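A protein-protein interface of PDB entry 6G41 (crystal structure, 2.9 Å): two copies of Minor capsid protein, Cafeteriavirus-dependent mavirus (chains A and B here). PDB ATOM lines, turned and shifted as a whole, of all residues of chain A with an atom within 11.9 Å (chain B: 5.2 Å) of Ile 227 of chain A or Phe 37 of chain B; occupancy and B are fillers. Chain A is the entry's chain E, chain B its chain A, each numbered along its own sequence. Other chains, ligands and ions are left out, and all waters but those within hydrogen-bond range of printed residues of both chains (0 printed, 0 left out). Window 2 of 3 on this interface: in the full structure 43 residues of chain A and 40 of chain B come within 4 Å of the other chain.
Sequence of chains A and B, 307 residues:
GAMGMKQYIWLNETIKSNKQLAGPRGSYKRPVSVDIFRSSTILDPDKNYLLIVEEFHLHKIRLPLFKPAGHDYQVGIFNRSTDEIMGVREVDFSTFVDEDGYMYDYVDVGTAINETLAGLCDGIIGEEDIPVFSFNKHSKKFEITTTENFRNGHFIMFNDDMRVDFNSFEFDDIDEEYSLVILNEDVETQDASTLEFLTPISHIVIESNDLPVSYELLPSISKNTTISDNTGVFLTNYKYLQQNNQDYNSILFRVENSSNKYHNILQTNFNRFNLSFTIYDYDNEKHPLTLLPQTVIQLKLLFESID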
ATOM      1  N   LEU A 217       4.989 -12.879  -9.397  1.00  0.00           N
ATOM      2  CA  LEU A 217       3.640 -12.540  -8.950  1.00  0.00           C
ATOM      3  C   LEU A 217       3.667 -12.337  -7.439  1.00  0.00           C
ATOM      4  O   LEU A 217       4.343 -13.080  -6.728  1.00  0.00           O
ATOM      5  CB  LEU A 217       2.625 -13.622  -9.331  1.00  0.00           C
ATOM      6  CG  LEU A 217       2.640 -14.146 -10.774  1.00  0.00           C
ATOM      7  CD1 LEU A 217       1.456 -15.074 -11.018  1.00  0.00           C
ATOM      8  CD2 LEU A 217       2.664 -13.011 -11.789  1.00  0.00           C
ATOM      9  N   LEU A 218       2.944 -11.321  -6.971  1.00  0.00           N
ATOM     10  CA  LEU A 218       2.910 -10.939  -5.559  1.00  0.00           C
ATOM     11  C   LEU A 218       1.463 -10.773  -5.080  1.00  0.00           C
ATOM     12  O   LEU A 218       0.560 -10.579  -5.896  1.00  0.00           O
ATOM     13  CB  LEU A 218       3.636  -9.601  -5.360  1.00  0.00           C
ATOM     14  CG  LEU A 218       5.161  -9.547  -5.277  1.00  0.00           C
ATOM     15  CD1 LEU A 218       5.614  -8.098  -5.323  1.00  0.00           C
ATOM     16  CD2 LEU A 218       5.661 -10.196  -4.001  1.00  0.00           C
ATOM     17  N   PRO A 219       1.240 -10.844  -3.754  1.00  0.00           N
ATOM     18  CA  PRO A 219      -0.082 -10.535  -3.207  1.00  0.00           C
ATOM     19  C   PRO A 219      -0.346  -9.026  -3.166  1.00  0.00           C
ATOM     20  O   PRO A 219       0.601  -8.231  -3.221  1.00  0.00           O
ATOM     21  CB  PRO A 219      -0.016 -11.123  -1.796  1.00  0.00           C
ATOM     22  CG  PRO A 219       1.426 -11.066  -1.430  1.00  0.00           C
ATOM     23  CD  PRO A 219       2.187 -11.272  -2.705  1.00  0.00           C
ATOM     24  N   SER A 220      -1.627  -8.656  -3.068  1.00  0.00           N
ATOM     25  CA  SER A 220      -2.067  -7.244  -3.080  1.00  0.00           C
ATOM     26  C   SER A 220      -1.448  -6.393  -1.979  1.00  0.00           C
ATOM     27  O   SER A 220      -1.163  -6.886  -0.884  1.00  0.00           O
ATOM     28  CB  SER A 220      -3.590  -7.132  -2.950  1.00  0.00           C
ATOM     29  OG  SER A 220      -4.220  -7.243  -4.203  1.00  0.00           O
ATOM     30  N   ILE A 221      -1.277  -5.106  -2.282  1.00  0.00           N
ATOM     31  CA  ILE A 221      -0.776  -4.121  -1.318  1.00  0.00           C
ATOM     32  C   ILE A 221      -1.794  -3.894  -0.191  1.00  0.00           C
ATOM     33  O   ILE A 221      -1.406  -3.724   0.972  1.00  0.00           O
ATOM     34  CB  ILE A 221      -0.411  -2.782  -2.018  1.00  0.00           C
ATOM     35  CG1 ILE A 221       0.747  -2.998  -3.008  1.00  0.00           C
ATOM     36  CG2 ILE A 221      -0.023  -1.696  -1.006  1.00  0.00           C
ATOM     37  CD1 ILE A 221       0.882  -1.924  -4.070  1.00  0.00           C
ATOM     38  N   SER A 222      -3.081  -3.899  -0.536  1.00  0.00           N
ATOM     39  CA  SER A 222      -4.152  -3.668   0.439  1.00  0.00           C
ATOM     40  C   SER A 222      -4.389  -4.861   1.371  1.00  0.00           C
ATOM     41  O   SER A 222      -4.384  -6.021   0.941  1.00  0.00           O
ATOM     42  CB  SER A 222      -5.462  -3.286  -0.266  1.00  0.00           C
ATOM     43  OG  SER A 222      -5.751  -4.161  -1.343  1.00  0.00           O
ATOM     44  N   LYS A 223      -4.602  -4.544   2.647  1.00  0.00           N
ATOM     45  CA  LYS A 223      -5.016  -5.516   3.669  1.00  0.00           C
ATOM     46  C   LYS A 223      -6.482  -5.941   3.475  1.00  0.00           C
ATOM     47  O   LYS A 223      -6.877  -7.041   3.871  1.00  0.00           O
ATOM     48  CB  LYS A 223      -4.871  -4.910   5.076  1.00  0.00           C
ATOM     49  CG  LYS A 223      -3.484  -4.385   5.445  1.00  0.00           C
ATOM     50  CD  LYS A 223      -2.632  -5.416   6.169  1.00  0.00           C
ATOM     51  CE  LYS A 223      -1.327  -4.801   6.653  1.00  0.00           C
ATOM     52  NZ  LYS A 223      -0.595  -5.687   7.603  1.00  0.00           N
ATOM     53  N   ASN A 224      -7.278  -5.051   2.878  1.00  0.00           N
ATOM     54  CA  ASN A 224      -8.722  -5.234   2.722  1.00  0.00           C
ATOM     55  C   ASN A 224      -9.121  -6.081   1.517  1.00  0.00           C
ATOM     56  O   ASN A 224     -10.142  -6.774   1.561  1.00  0.00           O
ATOM     57  CB  ASN A 224      -9.402  -3.868   2.600  1.00  0.00           C
ATOM     58  CG  ASN A 224      -9.287  -3.032   3.873  1.00  0.00           C
ATOM     59  OD1 ASN A 224      -9.516  -3.526   4.980  1.00  0.00           O
ATOM     60  ND2 ASN A 224      -8.956  -1.752   3.714  1.00  0.00           N
ATOM     61  N   THR A 225      -8.333  -5.999   0.445  1.00  0.00           N
ATOM     62  CA  THR A 225      -8.614  -6.699  -0.812  1.00  0.00           C
ATOM     63  C   THR A 225      -7.698  -7.924  -0.970  1.00  0.00           C
ATOM     64  O   THR A 225      -6.516  -7.868  -0.610  1.00  0.00           O
ATOM     65  CB  THR A 225      -8.422  -5.758  -2.028  1.00  0.00           C
ATOM     66  OG1 THR A 225      -8.888  -4.439  -1.717  1.00  0.00           O
ATOM     67  CG2 THR A 225      -9.174  -6.269  -3.221  1.00  0.00           C
ATOM     68  N   THR A 226      -8.254  -9.018  -1.500  1.00  0.00           N
ATOM     69  CA  THR A 226      -7.484 -10.237  -1.845  1.00  0.00           C
ATOM     70  C   THR A 226      -7.094 -10.278  -3.335  1.00  0.00           C
ATOM     71  O   THR A 226      -5.964 -10.655  -3.655  1.00  0.00           O
ATOM     72  CB  THR A 226      -8.250 -11.529  -1.467  1.00  0.00           C
ATOM     73  OG1 THR A 226      -8.566 -11.502  -0.073  1.00  0.00           O
ATOM     74  CG2 THR A 226      -7.421 -12.785  -1.743  1.00  0.00           C
ATOM     75  N   ILE A 227      -8.023  -9.915  -4.229  1.00  0.00           N
ATOM     76  CA  ILE A 227      -7.744  -9.841  -5.681  1.00  0.00           C
ATOM     77  C   ILE A 227      -6.455  -9.050  -5.985  1.00  0.00           C
ATOM     78  O   ILE A 227      -6.317  -7.890  -5.580  1.00  0.00           O
ATOM     79  CB  ILE A 227      -8.955  -9.310  -6.514  1.00  0.00           C
ATOM     80  CG1 ILE A 227      -8.641  -9.334  -8.021  1.00  0.00           C
ATOM     81  CG2 ILE A 227      -9.411  -7.925  -6.077  1.00  0.00           C
ATOM     82  CD1 ILE A 227      -9.866  -9.426  -8.909  1.00  0.00           C
ATOM     83  N   SER A 228      -5.523  -9.705  -6.680  1.00  0.00           N
ATOM     84  CA  SER A 228      -4.168  -9.188  -6.866  1.00  0.00           C
ATOM     85  C   SER A 228      -3.808  -8.944  -8.326  1.00  0.00           C
ATOM     86  O   SER A 228      -3.988  -9.801  -9.192  1.00  0.00           O
ATOM     87  CB  SER A 228      -3.135 -10.126  -6.239  1.00  0.00           C
ATOM     88  OG  SER A 228      -1.874  -9.479  -6.121  1.00  0.00           O
ATOM     89  N   ASP A 229      -3.299  -7.743  -8.562  1.00  0.00           N
ATOM     90  CA  ASP A 229      -2.704  -7.335  -9.824  1.00  0.00           C
ATOM     91  C   ASP A 229      -1.174  -7.244  -9.681  1.00  0.00           C
ATOM     92  O   ASP A 229      -0.462  -7.120 -10.675  1.00  0.00           O
ATOM     93  CB  ASP A 229      -3.272  -5.954 -10.185  1.00  0.00           C
ATOM     94  CG  ASP A 229      -3.523  -5.781 -11.667  1.00  0.00           C
ATOM     95  OD1 ASP A 229      -2.677  -6.201 -12.481  1.00  0.00           O
ATOM     96  OD2 ASP A 229      -4.573  -5.199 -12.011  1.00  0.00           O
ATOM     97  N   ASN A 230      -0.676  -7.334  -8.447  1.00  0.00           N
ATOM     98  CA  ASN A 230       0.653  -6.842  -8.106  1.00  0.00           C
ATOM     99  C   ASN A 230       1.772  -7.731  -8.641  1.00  0.00           C
ATOM    100  O   ASN A 230       1.597  -8.932  -8.815  1.00  0.00           O
ATOM    101  CB  ASN A 230       0.776  -6.699  -6.583  1.00  0.00           C
ATOM    102  CG  ASN A 230       1.884  -5.741  -6.157  1.00  0.00           C
ATOM    103  OD1 ASN A 230       2.353  -4.905  -6.936  1.00  0.00           O
ATOM    104  ND2 ASN A 230       2.293  -5.848  -4.899  1.00  0.00           N
ATOM    105  N   THR A 231       2.914  -7.111  -8.917  1.00  0.00           N
ATOM    106  CA  THR A 231       4.106  -7.797  -9.402  1.00  0.00           C
ATOM    107  C   THR A 231       5.360  -7.099  -8.878  1.00  0.00           C
ATOM    108  O   THR A 231       5.331  -5.916  -8.520  1.00  0.00           O
ATOM    109  CB  THR A 231       4.165  -7.830 -10.943  1.00  0.00           C
ATOM    110  OG1 THR A 231       3.944  -6.514 -11.464  1.00  0.00           O
ATOM    111  CG2 THR A 231       3.126  -8.784 -11.520  1.00  0.00           C
ATOM    112  N   ASP B  35      -5.776 -17.976   0.276  1.00  0.00           N
ATOM    113  CA  ASP B  35      -6.397 -17.828  -1.043  1.00  0.00           C
ATOM    114  C   ASP B  35      -5.471 -17.012  -1.929  1.00  0.00           C
ATOM    115  O   ASP B  35      -5.094 -15.894  -1.564  1.00  0.00           O
ATOM    116  CB  ASP B  35      -7.734 -17.086  -0.946  1.00  0.00           C
ATOM    117  CG  ASP B  35      -8.793 -17.861  -0.184  1.00  0.00           C
ATOM    118  OD1 ASP B  35      -8.667 -19.103  -0.048  1.00  0.00           O
ATOM    119  OD2 ASP B  35      -9.766 -17.215   0.273  1.00  0.00           O
ATOM    120  N   ILE B  36      -5.106 -17.570  -3.084  1.00  0.00           N
ATOM    121  CA  ILE B  36      -4.428 -16.801  -4.133  1.00  0.00           C
ATOM    122  C   ILE B  36      -5.453 -16.496  -5.222  1.00  0.00           C
ATOM    123  O   ILE B  36      -5.920 -17.396  -5.918  1.00  0.00           O
ATOM    124  CB  ILE B  36      -3.204 -17.517  -4.736  1.00  0.00           C
ATOM    125  CG1 ILE B  36      -2.196 -17.884  -3.642  1.00  0.00           C
ATOM    126  CG2 ILE B  36      -2.528 -16.611  -5.756  1.00  0.00           C
ATOM    127  CD1 ILE B  36      -2.360 -19.279  -3.094  1.00  0.00           C
ATOM    128  N   PHE B  37      -5.774 -15.213  -5.350  1.00  0.00           N
ATOM    129  CA  PHE B  37      -6.820 -14.716  -6.237  1.00  0.00           C
ATOM    130  C   PHE B  37      -6.193 -13.644  -7.116  1.00  0.00           C
ATOM    131  O   PHE B  37      -5.744 -12.611  -6.615  1.00  0.00           O
ATOM    132  CB  PHE B  37      -7.970 -14.142  -5.385  1.00  0.00           C
ATOM    133  CG  PHE B  37      -9.208 -13.755  -6.163  1.00  0.00           C
ATOM    134  CD1 PHE B  37      -9.743 -14.599  -7.120  1.00  0.00           C
ATOM    135  CD2 PHE B  37      -9.878 -12.568  -5.889  1.00  0.00           C
ATOM    136  CE1 PHE B  37     -10.892 -14.262  -7.822  1.00  0.00           C
ATOM    137  CE2 PHE B  37     -11.032 -12.221  -6.584  1.00  0.00           C
ATOM    138  CZ  PHE B  37     -11.539 -13.068  -7.553  1.00  0.00           C
ATOM    139  N   ARG B  38      -6.132 -13.905  -8.420  1.00  0.00           N
ATOM    140  CA  ARG B  38      -5.537 -12.962  -9.376  1.00  0.00           C
ATOM    141  C   ARG B  38      -6.556 -12.495 -10.418  1.00  0.00           C
ATOM    142  O   ARG B  38      -7.471 -13.239 -10.775  1.00  0.00           O
ATOM    143  CB  ARG B  38      -4.313 -13.590 -10.037  1.00  0.00           C
ATOM    144  CG  ARG B  38      -3.284 -14.055  -9.012  1.00  0.00           C
ATOM    145  CD  ARG B  38      -1.878 -14.164  -9.569  1.00  0.00           C
ATOM    146  NE  ARG B  38      -1.395 -12.902 -10.136  1.00  0.00           N
ATOM    147  CZ  ARG B  38      -0.827 -11.898  -9.462  1.00  0.00           C
ATOM    148  NH1 ARG B  38      -0.436 -10.813 -10.129  1.00  0.00           N
ATOM    149  NH2 ARG B  38      -0.640 -11.948  -8.143  1.00  0.00           N
ATOM    150  N   SER B  39      -6.401 -11.251 -10.871  1.00  0.00           N
ATOM    151  CA  SER B  39      -7.308 -10.650 -11.855  1.00  0.00           C
ATOM    152  C   SER B  39      -7.075 -11.249 -13.234  1.00  0.00           C
ATOM    153  O   SER B  39      -8.015 -11.679 -13.897  1.00  0.00           O
ATOM    154  CB  SER B  39      -7.135  -9.130 -11.900  1.00  0.00           C
ATOM    155  OG  SER B  39      -5.777  -8.772 -12.057  1.00  0.00           O
ATOM    156  N   ASN B 271      -7.613 -18.836 -12.013  1.00  0.00           N
ATOM    157  CA  ASN B 271      -7.040 -17.696 -11.293  1.00  0.00           C
ATOM    158  C   ASN B 271      -7.296 -17.705  -9.770  1.00  0.00           C
ATOM    159  O   ASN B 271      -6.889 -16.773  -9.076  1.00  0.00           O
ATOM    160  CB  ASN B 271      -7.566 -16.399 -11.912  1.00  0.00           C
ATOM    161  CG  ASN B 271      -9.063 -16.218 -11.717  1.00  0.00           C
ATOM    162  OD1 ASN B 271      -9.821 -17.189 -11.685  1.00  0.00           O
ATOM    163  ND2 ASN B 271      -9.496 -14.969 -11.586  1.00  0.00           N
ATOM    164  N   ARG B 272      -7.962 -18.748  -9.271  1.00  0.00           N
ATOM    165  CA  ARG B 272      -8.278 -18.925  -7.853  1.00  0.00           C
ATOM    166  C   ARG B 272      -7.718 -20.256  -7.399  1.00  0.00           C
ATOM    167  O   ARG B 272      -7.968 -21.272  -8.043  1.00  0.00           O
ATOM    168  CB  ARG B 272      -9.793 -19.031  -7.623  1.00  0.00           C
ATOM    169  CG  ARG B 272     -10.614 -17.798  -7.931  1.00  0.00           C
ATOM    170  CD  ARG B 272     -11.629 -17.448  -6.839  1.00  0.00           C
ATOM    171  NE  ARG B 272     -11.012 -17.194  -5.527  1.00  0.00           N
ATOM    172  CZ  ARG B 272     -11.558 -16.498  -4.526  1.00  0.00           C
ATOM    173  NH1 ARG B 272     -12.758 -15.930  -4.645  1.00  0.00           N
ATOM    174  NH2 ARG B 272     -10.883 -16.355  -3.385  1.00  0.00           N
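The backbone carbonyl oxygen of Leu 218 of chain A sits at hydrogen-bond distance from the guanidinium group of Arg 38 of chain B (2.9 Å).
N of Ser 39 of chain B is in hydrogen-bond range of O of Ser 228 of chain A (3.3 Å).
The guanidinium group (NH1) of Arg 38 of chain B is in hydrogen-bond range of the backbone carbonyl oxygen (O) of Asn 230 of chain A.
The side-chain hydroxyl (OG) of Ser 228 of chain A lies within hydrogen-bond range of the guanidinium group (NH2) of Arg 38 of chain B, at 3.4 Å.
O of Phe 37 of chain B sits at hydrogen-bond distance from N of Ser 228 of chain A (2.9 Å).
The backbone carbonyl oxygen (O) of Leu 218 of chain A sits at hydrogen-bond distance from the side-chain hydroxyl (OG) of Ser 228 of chain A (2.7 Å).
The backbone carbonyl oxygen (O) of Arg 38 of chain B sits at hydrogen-bond distance from the side-chain amide nitrogen (ND2) of Asn 271 of chain B, 2.8 Å away.
N of Asn 230 of chain A is in hydrogen-bond range of OG of Ser 228 of chain A, 3.4 Å away.
ND2 of Asn 230 of chain A lies within hydrogen-bond range of O of Pro 219 of chain A.
The backbone NH of Ser 220 of chain A is in hydrogen-bond range of the side-chain hydroxyl of Ser 228 of chain A (3.2 Å).
The backbone carbonyl oxygen of Asn 230 of chain A sits at hydrogen-bond distance from the backbone NH of Leu 218 of chain A (3.3 Å).
Arg 38 of chain B touches Leu 217 of chain A (NE to CD1, 3.7 Å).
O of Asp 35 of chain B touches CG2 of Thr 226 of chain A, at 3.9 Å.
Phe 37 of chain B touches Thr 226 of chain A.
CB of Ile 227 of chain A touches CD2 of Phe 37 of chain B, at 3.4 Å.
Asp 229 of chain A touches Arg 38 of chain B (C to NH1, 3.7 Å).
Ser 39 of chain B touches Asp 229 of chain A.
Of the printed residues of chain B, Thr 226 of chain A touches Asp 35 (3.9 Å) and Phe 37 (3.6 Å).
Ile 227 of chain A touches one residue of chain B.
Printed residues of chain B within 4 Å of Ser 228 of chain A: Phe 37, Arg 38 and Ser 39.
Of the printed residues of chain A, Asp 35 of chain B touches Thr 226 (3.9 Å).
No residue of chain A comes within 4 Å of Asn 271 of chain B.
Arg 272 of chain B touches none of the printed residues of chain A.
The nearest residue of chain B that does not touch Ile 227 of chain A is Ser 39 of chain B (4.1 Å).
The nearest printed residue of chain B that does not touch Asn 230 of chain A is Ser 39 of chain B (6.4 Å).
Of the 15 printed residues of chain A, 7 touch a printed residue of chain B.
Printed residues of chain A that touch a printed residue of chain B: Leu 217, Leu 218, Thr 226, Ile 227, Ser 228, Asp 229 and Asn 230.
Hydrophobic or aromatic side chains of chain A within 4 Å of the printed part of chain B: Leu 217 and Ile 227.
Of the 7 printed residues of chain B, 4 touch a printed residue of chain A.
Among the printed residues, no Asp or Glu carboxylate lies within 4 Å of a Lys or Arg side-chain nitrogen of the other chain.
No position is printed for both chains.
Of the 11 pairs that touch across the chains among the printed residues, none has its exchanged pair printed and touching as well.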
